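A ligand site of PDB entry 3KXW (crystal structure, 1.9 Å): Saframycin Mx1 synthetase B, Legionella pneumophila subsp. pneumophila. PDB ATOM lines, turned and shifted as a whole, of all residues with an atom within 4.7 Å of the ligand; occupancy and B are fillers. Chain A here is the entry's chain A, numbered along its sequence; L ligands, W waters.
A nitrogen (N4) of the ligand lies close to the backbone carbonyl oxygen of Glu 299, 3.4 Å away.
Merely in contact with the ligand: Ile 199, Phe 203, Met 205, Met 221, Gly 225, Phe 295, Pro 300, Val 301, Tyr 327, Gly 328, Leu 329, Leu 334, Leu 335, Val 453 and Arg 456.
Hydrophobic or aromatic side chains that line the ligand: Ile 199, Phe 203, Met 205, His 219, Met 221, Phe 295, Ala 298, Val 301, Tyr 327, Leu 329, Ala 330, Leu 334, Leu 335 and Val 453.
Water W2 lies within hydrogen-bond range of a nitrogen (N4) of the ligand and the backbone NH of Val 301.
Water W4 bridges an oxygen (O8) of the ligand and the guanidinium group (NH1) of Arg 456.
Water W5 lies within hydrogen-bond range of OE1 of Glu 331 (2.8 Å) and O3 of the ligand (3.0 Å).
Water W1 bridges the backbone carbonyl oxygen of Ala 298 (2.8 Å) and an oxygen (O5) of the ligand (3.1 Å).
Water W6 bridges the backbone NH of Asp 220 (2.9 Å) and an oxygen (O4) of the ligand (3.3 Å).
The side-chain hydroxyl (OG) of Ser 376 sits at hydrogen-bond distance from a nitrogen (N5) of the ligand, 3.0 Å away.
OD2 of Asp 220 lies close to O2 of the ligand (2.4 Å).
O3 of the ligand is in hydrogen-bond range of N of Ala 330 (3.0 Å).
A nitrogen (N5) of the ligand lies within hydrogen-bond range of the backbone carbonyl oxygen (O) of Cys 326, 2.9 Å away.
The side-chain carboxylate (OD2) of Asp 442 lies within hydrogen-bond range of an oxygen (O8) of the ligand (2.7 Å).
N of Ala 298 sits at hydrogen-bond distance from N2 of the ligand, 3.2 Å away.
O4 of the ligand is in hydrogen-bond range of NE2 of His 219.
The backbone NH (N) of Met 221 sits at hydrogen-bond distance from a ring nitrogen (ND1) of His 219 (3.2 Å).
N of Cys 226 lies within hydrogen-bond range of O of Met 221, 3.2 Å away.
The side-chain carboxylate (OD2) of Asp 442 sits at hydrogen-bond distance from the side-chain hydroxyl (OH) of Tyr 327.
The backbone NH (N) of Leu 329 sits at hydrogen-bond distance from the backbone carbonyl oxygen (O) of Leu 334, 3.2 Å away.
The side-chain carboxylate of Asp 442 lies within salt-bridge range of the guanidinium group of Arg 456, at 2.8 Å.
The guanidinium group (NH1) of Arg 456 sits at hydrogen-bond distance from the backbone carbonyl oxygen (O) of Thr 440, 3.0 Å away.
The side-chain hydroxyl (OG1) of Thr 440 is in hydrogen-bond range of the backbone NH (N) of Asp 442 (3.0 Å).
N of Ala 330 lies within hydrogen-bond range of OD2 of Asp 220, at 3.2 Å.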
ATOM      1  N   THR A 175     -20.002 -10.016   3.338  1.00  0.00           N
ATOM      2  CA  THR A 175     -21.416  -9.964   2.989  1.00  0.00           C
ATOM      3  C   THR A 175     -21.917  -8.546   3.176  1.00  0.00           C
ATOM      4  O   THR A 175     -21.236  -7.722   3.784  1.00  0.00           O
ATOM      5  CB  THR A 175     -22.261 -10.883   3.863  1.00  0.00           C
ATOM      6  OG1 THR A 175     -22.128 -10.481   5.228  1.00  0.00           O
ATOM      7  CG2 THR A 175     -21.793 -12.317   3.729  1.00  0.00           C
ATOM      8  N   SER A 176     -23.115  -8.270   2.670  1.00  0.00           N
ATOM      9  CA  SER A 176     -23.762  -7.006   3.003  1.00  0.00           C
ATOM     10  C   SER A 176     -24.327  -7.134   4.417  1.00  0.00           C
ATOM     11  O   SER A 176     -24.357  -8.232   5.005  1.00  0.00           O
ATOM     12  CB  SER A 176     -24.895  -6.682   2.024  1.00  0.00           C
ATOM     13  OG  SER A 176     -25.950  -7.615   2.157  1.00  0.00           O
ATOM     14  N   ILE A 199     -22.797 -25.517  -9.399  1.00  0.00           N
ATOM     15  CA  ILE A 199     -23.295 -24.503 -10.337  1.00  0.00           C
ATOM     16  C   ILE A 199     -23.222 -24.990 -11.796  1.00  0.00           C
ATOM     17  O   ILE A 199     -24.210 -24.924 -12.540  1.00  0.00           O
ATOM     18  CB  ILE A 199     -22.519 -23.165 -10.187  1.00  0.00           C
ATOM     19  CG1 ILE A 199     -22.683 -22.610  -8.766  1.00  0.00           C
ATOM     20  CG2 ILE A 199     -22.954 -22.143 -11.248  1.00  0.00           C
ATOM     21  CD1 ILE A 199     -21.761 -21.429  -8.435  1.00  0.00           C
ATOM     22  N   PHE A 203     -26.837 -25.798 -13.562  1.00  0.00           N
ATOM     23  CA  PHE A 203     -27.156 -24.903 -14.689  1.00  0.00           C
ATOM     24  C   PHE A 203     -27.046 -25.590 -16.061  1.00  0.00           C
ATOM     25  O   PHE A 203     -27.169 -24.941 -17.087  1.00  0.00           O
ATOM     26  CB  PHE A 203     -26.306 -23.617 -14.665  1.00  0.00           C
ATOM     27  CG  PHE A 203     -26.817 -22.565 -13.709  1.00  0.00           C
ATOM     28  CD1 PHE A 203     -26.863 -22.802 -12.332  1.00  0.00           C
ATOM     29  CD2 PHE A 203     -27.267 -21.332 -14.184  1.00  0.00           C
ATOM     30  CE1 PHE A 203     -27.361 -21.828 -11.437  1.00  0.00           C
ATOM     31  CE2 PHE A 203     -27.764 -20.359 -13.288  1.00  0.00           C
ATOM     32  CZ  PHE A 203     -27.804 -20.615 -11.919  1.00  0.00           C
ATOM     33  N   MET A 205     -24.562 -26.522 -17.804  1.00  0.00           N
ATOM     34  CA  MET A 205     -23.563 -25.897 -18.650  1.00  0.00           C
ATOM     35  C   MET A 205     -22.922 -26.916 -19.573  1.00  0.00           C
ATOM     36  O   MET A 205     -22.836 -28.087 -19.220  1.00  0.00           O
ATOM     37  CB  MET A 205     -22.475 -25.231 -17.797  1.00  0.00           C
ATOM     38  CG  MET A 205     -23.056 -24.153 -16.925  1.00  0.00           C
ATOM     39  SD  MET A 205     -21.718 -22.943 -16.184  1.00  0.00           S
ATOM     40  CE  MET A 205     -22.954 -21.903 -15.099  1.00  0.00           C
ATOM     41  N   ILE A 211     -21.498 -17.116 -20.726  1.00  0.00           N
ATOM     42  CA  ILE A 211     -22.097 -16.351 -19.648  1.00  0.00           C
ATOM     43  C   ILE A 211     -21.906 -14.863 -19.869  1.00  0.00           C
ATOM     44  O   ILE A 211     -20.814 -14.416 -20.208  1.00  0.00           O
ATOM     45  CB  ILE A 211     -21.511 -16.770 -18.289  1.00  0.00           C
ATOM     46  CG1 ILE A 211     -21.805 -18.259 -18.025  1.00  0.00           C
ATOM     47  CG2 ILE A 211     -22.013 -15.855 -17.173  1.00  0.00           C
ATOM     48  CD1 ILE A 211     -21.155 -18.803 -16.742  1.00  0.00           C
ATOM     49  N   HIS A 219     -19.483  -9.106  -4.899  1.00  0.00           N
ATOM     50  CA  HIS A 219     -20.559  -9.851  -4.246  1.00  0.00           C
ATOM     51  C   HIS A 219     -20.410 -11.305  -4.754  1.00  0.00           C
ATOM     52  O   HIS A 219     -19.957 -11.536  -5.863  1.00  0.00           O
ATOM     53  CB  HIS A 219     -21.900  -9.230  -4.667  1.00  0.00           C
ATOM     54  CG  HIS A 219     -23.104  -9.979  -4.172  1.00  0.00           C
ATOM     55  ND1 HIS A 219     -23.745 -10.937  -4.933  1.00  0.00           N
ATOM     56  CD2 HIS A 219     -23.784  -9.902  -3.006  1.00  0.00           C
ATOM     57  CE1 HIS A 219     -24.767 -11.419  -4.248  1.00  0.00           C
ATOM     58  NE2 HIS A 219     -24.811 -10.809  -3.079  1.00  0.00           N
ATOM     59  N   ASP A 220     -20.758 -12.276  -3.915  1.00  0.00           N
ATOM     60  CA  ASP A 220     -20.648 -13.684  -4.287  1.00  0.00           C
ATOM     61  C   ASP A 220     -21.204 -14.077  -5.674  1.00  0.00           C
ATOM     62  O   ASP A 220     -20.531 -14.769  -6.411  1.00  0.00           O
ATOM     63  CB  ASP A 220     -21.235 -14.594  -3.188  1.00  0.00           C
ATOM     64  CG  ASP A 220     -22.662 -14.249  -2.830  1.00  0.00           C
ATOM     65  OD1 ASP A 220     -23.302 -13.483  -3.599  1.00  0.00           O
ATOM     66  OD2 ASP A 220     -23.144 -14.760  -1.789  1.00  0.00           O
ATOM     67  N   MET A 221     -22.412 -13.654  -6.019  1.00  0.00           N
ATOM     68  CA  MET A 221     -22.992 -14.074  -7.291  1.00  0.00           C
ATOM     69  C   MET A 221     -22.156 -13.691  -8.524  1.00  0.00           C
ATOM     70  O   MET A 221     -21.887 -14.532  -9.393  1.00  0.00           O
ATOM     71  CB  MET A 221     -24.412 -13.499  -7.420  1.00  0.00           C
ATOM     72  CG  MET A 221     -25.310 -14.328  -8.264  1.00  0.00           C
ATOM     73  SD  MET A 221     -27.247 -14.042  -7.857  1.00  0.00           S
ATOM     74  CE  MET A 221     -27.254 -12.124  -8.174  1.00  0.00           C
ATOM     75  N   GLY A 225     -20.415 -17.177  -9.259  1.00  0.00           N
ATOM     76  CA  GLY A 225     -21.246 -17.605 -10.363  1.00  0.00           C
ATOM     77  C   GLY A 225     -20.741 -17.194 -11.734  1.00  0.00           C
ATOM     78  O   GLY A 225     -20.673 -18.019 -12.640  1.00  0.00           O
ATOM     79  N   CYS A 226     -20.398 -15.933 -11.907  1.00  0.00           N
ATOM     80  CA  CYS A 226     -20.219 -15.417 -13.265  1.00  0.00           C
ATOM     81  C   CYS A 226     -18.749 -15.261 -13.713  1.00  0.00           C
ATOM     82  O   CYS A 226     -18.481 -14.942 -14.854  1.00  0.00           O
ATOM     83  CB  CYS A 226     -20.967 -14.096 -13.432  1.00  0.00           C
ATOM     84  SG  CYS A 226     -22.730 -14.291 -13.093  1.00  0.00           S
ATOM     85  N   ILE A 263     -26.425 -17.924 -20.575  1.00  0.00           N
ATOM     86  CA  ILE A 263     -26.712 -17.762 -19.157  1.00  0.00           C
ATOM     87  C   ILE A 263     -26.380 -16.349 -18.714  1.00  0.00           C
ATOM     88  O   ILE A 263     -25.300 -15.856 -18.989  1.00  0.00           O
ATOM     89  CB  ILE A 263     -25.892 -18.742 -18.322  1.00  0.00           C
ATOM     90  CG1 ILE A 263     -26.164 -20.179 -18.792  1.00  0.00           C
ATOM     91  CG2 ILE A 263     -26.259 -18.615 -16.857  1.00  0.00           C
ATOM     92  CD1 ILE A 263     -25.386 -21.219 -17.968  1.00  0.00           C
ATOM     93  N   PHE A 295     -31.157 -16.267 -14.661  1.00  0.00           N
ATOM     94  CA  PHE A 295     -31.303 -16.600 -13.238  1.00  0.00           C
ATOM     95  C   PHE A 295     -31.717 -15.379 -12.419  1.00  0.00           C
ATOM     96  O   PHE A 295     -31.461 -14.242 -12.795  1.00  0.00           O
ATOM     97  CB  PHE A 295     -30.069 -17.307 -12.672  1.00  0.00           C
ATOM     98  CG  PHE A 295     -28.827 -16.446 -12.668  1.00  0.00           C
ATOM     99  CD1 PHE A 295     -27.913 -16.527 -13.717  1.00  0.00           C
ATOM    100  CD2 PHE A 295     -28.582 -15.600 -11.610  1.00  0.00           C
ATOM    101  CE1 PHE A 295     -26.767 -15.724 -13.713  1.00  0.00           C
ATOM    102  CE2 PHE A 295     -27.445 -14.800 -11.595  1.00  0.00           C
ATOM    103  CZ  PHE A 295     -26.537 -14.859 -12.627  1.00  0.00           C
ATOM    104  N   GLY A 297     -31.825 -14.432  -8.408  1.00  0.00           N
ATOM    105  CA  GLY A 297     -31.494 -14.762  -7.026  1.00  0.00           C
ATOM    106  C   GLY A 297     -30.813 -13.601  -6.314  1.00  0.00           C
ATOM    107  O   GLY A 297     -30.355 -12.661  -6.970  1.00  0.00           O
ATOM    108  N   ALA A 298     -30.716 -13.714  -4.988  1.00  0.00           N
ATOM    109  CA  ALA A 298     -30.015 -12.801  -4.080  1.00  0.00           C
ATOM    110  C   ALA A 298     -30.989 -11.944  -3.269  1.00  0.00           C
ATOM    111  O   ALA A 298     -30.594 -11.290  -2.298  1.00  0.00           O
ATOM    112  CB  ALA A 298     -28.976 -11.938  -4.789  1.00  0.00           C
ATOM    113  N   GLU A 299     -32.246 -11.978  -3.661  1.00  0.00           N
ATOM    114  CA  GLU A 299     -33.278 -11.242  -2.942  1.00  0.00           C
ATOM    115  C   GLU A 299     -34.621 -11.843  -3.303  1.00  0.00           C
ATOM    116  O   GLU A 299     -34.706 -12.709  -4.161  1.00  0.00           O
ATOM    117  CB  GLU A 299     -33.246  -9.757  -3.301  1.00  0.00           C
ATOM    118  CG  GLU A 299     -33.685  -9.464  -4.736  1.00  0.00           C
ATOM    119  CD  GLU A 299     -33.484  -8.003  -5.105  1.00  0.00           C
ATOM    120  OE1 GLU A 299     -32.701  -7.323  -4.409  1.00  0.00           O
ATOM    121  OE2 GLU A 299     -34.112  -7.537  -6.065  1.00  0.00           O
ATOM    122  N   PRO A 300     -35.697 -11.381  -2.657  1.00  0.00           N
ATOM    123  CA  PRO A 300     -36.966 -12.054  -2.959  1.00  0.00           C
ATOM    124  C   PRO A 300     -37.339 -12.033  -4.439  1.00  0.00           C
ATOM    125  O   PRO A 300     -37.229 -11.024  -5.117  1.00  0.00           O
ATOM    126  CB  PRO A 300     -37.973 -11.301  -2.103  1.00  0.00           C
ATOM    127  CG  PRO A 300     -37.166 -10.853  -0.941  1.00  0.00           C
ATOM    128  CD  PRO A 300     -35.825 -10.462  -1.520  1.00  0.00           C
ATOM    129  N   VAL A 301     -37.752 -13.181  -4.926  1.00  0.00           N
ATOM    130  CA  VAL A 301     -38.039 -13.378  -6.336  1.00  0.00           C
ATOM    131  C   VAL A 301     -39.551 -13.154  -6.576  1.00  0.00           C
ATOM    132  O   VAL A 301     -40.397 -13.765  -5.897  1.00  0.00           O
ATOM    133  CB  VAL A 301     -37.594 -14.802  -6.734  1.00  0.00           C
ATOM    134  CG1 VAL A 301     -38.060 -15.153  -8.149  1.00  0.00           C
ATOM    135  CG2 VAL A 301     -36.067 -14.961  -6.544  1.00  0.00           C
ATOM    136  N   CYS A 326     -33.355 -18.953  -7.947  1.00  0.00           N
ATOM    137  CA  CYS A 326     -32.409 -19.764  -7.178  1.00  0.00           C
ATOM    138  C   CYS A 326     -32.141 -19.069  -5.857  1.00  0.00           C
ATOM    139  O   CYS A 326     -32.355 -17.863  -5.737  1.00  0.00           O
ATOM    140  CB  CYS A 326     -31.096 -19.970  -7.957  1.00  0.00           C
ATOM    141  SG  CYS A 326     -30.391 -18.513  -8.751  1.00  0.00           S
ATOM    142  N   TYR A 327     -31.652 -19.824  -4.894  1.00  0.00           N
ATOM    143  CA  TYR A 327     -31.409 -19.287  -3.551  1.00  0.00           C
ATOM    144  C   TYR A 327     -30.007 -19.664  -3.095  1.00  0.00           C
ATOM    145  O   TYR A 327     -29.504 -20.716  -3.455  1.00  0.00           O
ATOM    146  CB  TYR A 327     -32.439 -19.863  -2.569  1.00  0.00           C
ATOM    147  CG  TYR A 327     -32.053 -19.718  -1.103  1.00  0.00           C
ATOM    148  CD1 TYR A 327     -32.269 -18.536  -0.415  1.00  0.00           C
ATOM    149  CD2 TYR A 327     -31.467 -20.785  -0.412  1.00  0.00           C
ATOM    150  CE1 TYR A 327     -31.917 -18.409   0.933  1.00  0.00           C
ATOM    151  CE2 TYR A 327     -31.123 -20.641   0.923  1.00  0.00           C
ATOM    152  CZ  TYR A 327     -31.358 -19.470   1.584  1.00  0.00           C
ATOM    153  OH  TYR A 327     -31.000 -19.364   2.914  1.00  0.00           O
ATOM    154  N   GLY A 328     -29.369 -18.784  -2.343  1.00  0.00           N
ATOM    155  CA  GLY A 328     -28.085 -19.102  -1.752  1.00  0.00           C
ATOM    156  C   GLY A 328     -27.574 -17.946  -0.904  1.00  0.00           C
ATOM    157  O   GLY A 328     -28.258 -16.935  -0.747  1.00  0.00           O
ATOM    158  N   LEU A 329     -26.384 -18.132  -0.349  1.00  0.00           N
ATOM    159  CA  LEU A 329     -25.753 -17.105   0.474  1.00  0.00           C
ATOM    160  C   LEU A 329     -24.256 -17.372   0.589  1.00  0.00           C
ATOM    161  O   LEU A 329     -23.795 -18.489   0.350  1.00  0.00           O
ATOM    162  CB  LEU A 329     -26.362 -16.971   1.872  1.00  0.00           C
ATOM    163  CG  LEU A 329     -26.916 -18.063   2.794  1.00  0.00           C
ATOM    164  CD1 LEU A 329     -26.746 -19.534   2.348  1.00  0.00           C
ATOM    165  CD2 LEU A 329     -26.605 -17.827   4.279  1.00  0.00           C
ATOM    166  N   ALA A 330     -23.510 -16.339   0.964  1.00  0.00           N
ATOM    167  CA  ALA A 330     -22.048 -16.420   0.952  1.00  0.00           C
ATOM    168  C   ALA A 330     -21.556 -17.499   1.910  1.00  0.00           C
ATOM    169  O   ALA A 330     -20.550 -18.130   1.652  1.00  0.00           O
ATOM    170  CB  ALA A 330     -21.465 -15.093   1.330  1.00  0.00           C
ATOM    171  N   GLU A 331     -22.282 -17.683   3.022  1.00  0.00           N
ATOM    172  CA  GLU A 331     -21.909 -18.656   4.058  1.00  0.00           C
ATOM    173  C   GLU A 331     -21.952 -20.090   3.521  1.00  0.00           C
ATOM    174  O   GLU A 331     -21.347 -21.002   4.099  1.00  0.00           O
ATOM    175  CB  GLU A 331     -22.802 -18.510   5.300  1.00  0.00           C
ATOM    176  CG  GLU A 331     -22.468 -17.282   6.141  1.00  0.00           C
ATOM    177  CD  GLU A 331     -23.218 -16.041   5.692  1.00  0.00           C
ATOM    178  OE1 GLU A 331     -23.691 -16.007   4.527  1.00  0.00           O
ATOM    179  OE2 GLU A 331     -23.341 -15.086   6.511  1.00  0.00           O
ATOM    180  N   LEU A 334     -22.164 -20.268  -2.418  1.00  0.00           N
ATOM    181  CA  LEU A 334     -23.127 -19.534  -3.236  1.00  0.00           C
ATOM    182  C   LEU A 334     -24.414 -20.302  -3.383  1.00  0.00           C
ATOM    183  O   LEU A 334     -25.366 -20.041  -2.661  1.00  0.00           O
ATOM    184  CB  LEU A 334     -22.563 -19.198  -4.618  1.00  0.00           C
ATOM    185  CG  LEU A 334     -23.476 -18.287  -5.462  1.00  0.00           C
ATOM    186  CD1 LEU A 334     -23.557 -16.881  -4.858  1.00  0.00           C
ATOM    187  CD2 LEU A 334     -22.937 -18.236  -6.884  1.00  0.00           C
ATOM    188  N   LEU A 335     -24.450 -21.254  -4.300  1.00  0.00           N
ATOM    189  CA  LEU A 335     -25.742 -21.833  -4.726  1.00  0.00           C
ATOM    190  C   LEU A 335     -26.231 -22.922  -3.796  1.00  0.00           C
ATOM    191  O   LEU A 335     -25.513 -23.889  -3.556  1.00  0.00           O
ATOM    192  CB  LEU A 335     -25.596 -22.396  -6.156  1.00  0.00           C
ATOM    193  CG  LEU A 335     -26.796 -23.114  -6.756  1.00  0.00           C
ATOM    194  CD1 LEU A 335     -28.004 -22.145  -6.955  1.00  0.00           C
ATOM    195  CD2 LEU A 335     -26.377 -23.785  -8.076  1.00  0.00           C
ATOM    196  N   SER A 376     -37.860 -21.236  -5.136  1.00  0.00           N
ATOM    197  CA  SER A 376     -36.425 -21.092  -5.400  1.00  0.00           C
ATOM    198  C   SER A 376     -35.776 -22.411  -5.837  1.00  0.00           C
ATOM    199  O   SER A 376     -34.558 -22.492  -5.963  1.00  0.00           O
ATOM    200  CB  SER A 376     -35.673 -20.486  -4.188  1.00  0.00           C
ATOM    201  OG  SER A 376     -36.005 -19.122  -4.007  1.00  0.00           O
ATOM    202  N   THR A 440     -29.103 -19.971   8.339  1.00  0.00           N
ATOM    203  CA  THR A 440     -29.048 -18.870   7.367  1.00  0.00           C
ATOM    204  C   THR A 440     -29.639 -17.554   7.853  1.00  0.00           C
ATOM    205  O   THR A 440     -29.357 -16.498   7.276  1.00  0.00           O
ATOM    206  CB  THR A 440     -29.747 -19.263   6.063  1.00  0.00           C
ATOM    207  OG1 THR A 440     -31.144 -19.481   6.317  1.00  0.00           O
ATOM    208  CG2 THR A 440     -29.133 -20.565   5.524  1.00  0.00           C
ATOM    209  N   ASP A 442     -32.655 -17.076   7.339  1.00  0.00           N
ATOM    210  CA  ASP A 442     -33.775 -17.010   6.405  1.00  0.00           C
ATOM    211  C   ASP A 442     -34.924 -17.921   6.820  1.00  0.00           C
ATOM    212  O   ASP A 442     -34.698 -19.008   7.330  1.00  0.00           O
ATOM    213  CB  ASP A 442     -33.301 -17.412   5.006  1.00  0.00           C
ATOM    214  CG  ASP A 442     -32.300 -16.448   4.436  1.00  0.00           C
ATOM    215  OD1 ASP A 442     -32.517 -15.231   4.564  1.00  0.00           O
ATOM    216  OD2 ASP A 442     -31.287 -16.904   3.851  1.00  0.00           O
ATOM    217  N   VAL A 453     -38.871 -19.373  -0.061  1.00  0.00           N
ATOM    218  CA  VAL A 453     -38.337 -18.428   0.917  1.00  0.00           C
ATOM    219  C   VAL A 453     -39.408 -17.396   1.292  1.00  0.00           C
ATOM    220  O   VAL A 453     -40.035 -16.799   0.425  1.00  0.00           O
ATOM    221  CB  VAL A 453     -37.062 -17.733   0.378  1.00  0.00           C
ATOM    222  CG1 VAL A 453     -36.496 -16.746   1.420  1.00  0.00           C
ATOM    223  CG2 VAL A 453     -36.017 -18.756  -0.018  1.00  0.00           C
ATOM    224  N   ARG A 456     -37.011 -13.074   6.515  1.00  0.00           N
ATOM    225  CA  ARG A 456     -35.878 -13.182   7.424  1.00  0.00           C
ATOM    226  C   ARG A 456     -36.423 -13.336   8.821  1.00  0.00           C
ATOM    227  O   ARG A 456     -37.508 -12.858   9.121  1.00  0.00           O
ATOM    228  CB  ARG A 456     -35.032 -11.895   7.387  1.00  0.00           C
ATOM    229  CG  ARG A 456     -34.338 -11.576   6.075  1.00  0.00           C
ATOM    230  CD  ARG A 456     -33.040 -12.345   5.901  1.00  0.00           C
ATOM    231  NE  ARG A 456     -32.068 -12.124   6.990  1.00  0.00           N
ATOM    232  CZ  ARG A 456     -31.012 -12.912   7.207  1.00  0.00           C
ATOM    233  NH1 ARG A 456     -30.796 -13.966   6.430  1.00  0.00           N
ATOM    234  NH2 ARG A 456     -30.187 -12.661   8.204  1.00  0.00           N
HETATM  235  P1  LIG L   1     -25.397 -12.926   0.076  1.00  0.00           P
HETATM  236  C1  LIG L   1     -23.763 -18.796 -13.221  1.00  0.00           C
HETATM  237  N1  LIG L   1     -31.619 -14.303  -0.766  1.00  0.00           N
HETATM  238  O1  LIG L   1     -27.317 -13.423  -2.509  1.00  0.00           O
HETATM  239  C2  LIG L   1     -24.622 -18.060 -12.183  1.00  0.00           C
HETATM  240  N2  LIG L   1     -31.549 -15.602  -2.576  1.00  0.00           N
HETATM  241  O2  LIG L   1     -25.313 -13.780  -1.342  1.00  0.00           O
HETATM  242  C3  LIG L   1     -25.008 -18.947 -11.001  1.00  0.00           C
HETATM  243  N3  LIG L   1     -34.226 -14.224  -0.487  1.00  0.00           N
HETATM  244  O3  LIG L   1     -24.586 -13.586   1.079  1.00  0.00           O
HETATM  245  C4  LIG L   1     -25.459 -18.100  -9.806  1.00  0.00           C
HETATM  246  N4  LIG L   1     -35.337 -15.467  -2.228  1.00  0.00           N
HETATM  247  O4  LIG L   1     -24.859 -11.434  -0.214  1.00  0.00           O
HETATM  248  C5  LIG L   1     -26.260 -18.905  -8.768  1.00  0.00           C
HETATM  249  N5  LIG L   1     -34.252 -16.705  -3.887  1.00  0.00           N
HETATM  250  O5  LIG L   1     -26.983 -12.781   0.606  1.00  0.00           O
HETATM  251  C6  LIG L   1     -26.771 -17.946  -7.698  1.00  0.00           C
HETATM  252  O6  LIG L   1     -29.793 -12.970   0.250  1.00  0.00           O
HETATM  253  C7  LIG L   1     -27.744 -18.385  -6.575  1.00  0.00           C
HETATM  254  O7  LIG L   1     -31.522 -13.658   2.485  1.00  0.00           O
HETATM  255  C8  LIG L   1     -28.326 -17.318  -5.620  1.00  0.00           C
HETATM  256  O8  LIG L   1     -29.528 -15.045   2.977  1.00  0.00           O
HETATM  257  C9  LIG L   1     -27.308 -17.043  -4.499  1.00  0.00           C
HETATM  258  C10 LIG L   1     -27.378 -15.614  -3.919  1.00  0.00           C
HETATM  259  C11 LIG L   1     -26.130 -15.399  -3.017  1.00  0.00           C
HETATM  260  C12 LIG L   1     -26.476 -14.364  -1.932  1.00  0.00           C
HETATM  261  C13 LIG L   1     -27.799 -13.921   0.773  1.00  0.00           C
HETATM  262  C14 LIG L   1     -29.077 -13.535   1.182  1.00  0.00           C
HETATM  263  C15 LIG L   1     -29.931 -14.724   1.740  1.00  0.00           C
HETATM  264  C16 LIG L   1     -31.183 -14.307   1.649  1.00  0.00           C
HETATM  265  C17 LIG L   1     -31.140 -13.640   0.363  1.00  0.00           C
HETATM  266  C18 LIG L   1     -30.799 -14.982  -1.750  1.00  0.00           C
HETATM  267  C19 LIG L   1     -32.960 -15.322  -2.180  1.00  0.00           C
HETATM  268  C20 LIG L   1     -32.985 -14.607  -1.097  1.00  0.00           C
HETATM  269  C21 LIG L   1     -35.361 -14.589  -1.047  1.00  0.00           C
HETATM  270  C22 LIG L   1     -34.275 -15.811  -2.759  1.00  0.00           C
HETATM  271  O   HOH W   1     -28.157 -10.519  -1.187  1.00  0.00           O
HETATM  272  O   HOH W   2     -37.724 -15.650  -3.200  1.00  0.00           O
HETATM  273  O   HOH W   3     -34.945 -12.707   1.581  1.00  0.00           O
HETATM  274  O   HOH W   4     -27.796 -13.976   4.880  1.00  0.00           O
HETATM  275  O   HOH W   5     -25.339 -13.806   3.974  1.00  0.00           O
HETATM  276  O   HOH W   6     -21.728 -11.823  -1.169  1.00  0.00           O
HETATM  277  O   HOH W   7     -31.060 -10.927   2.903  1.00  0.00           O
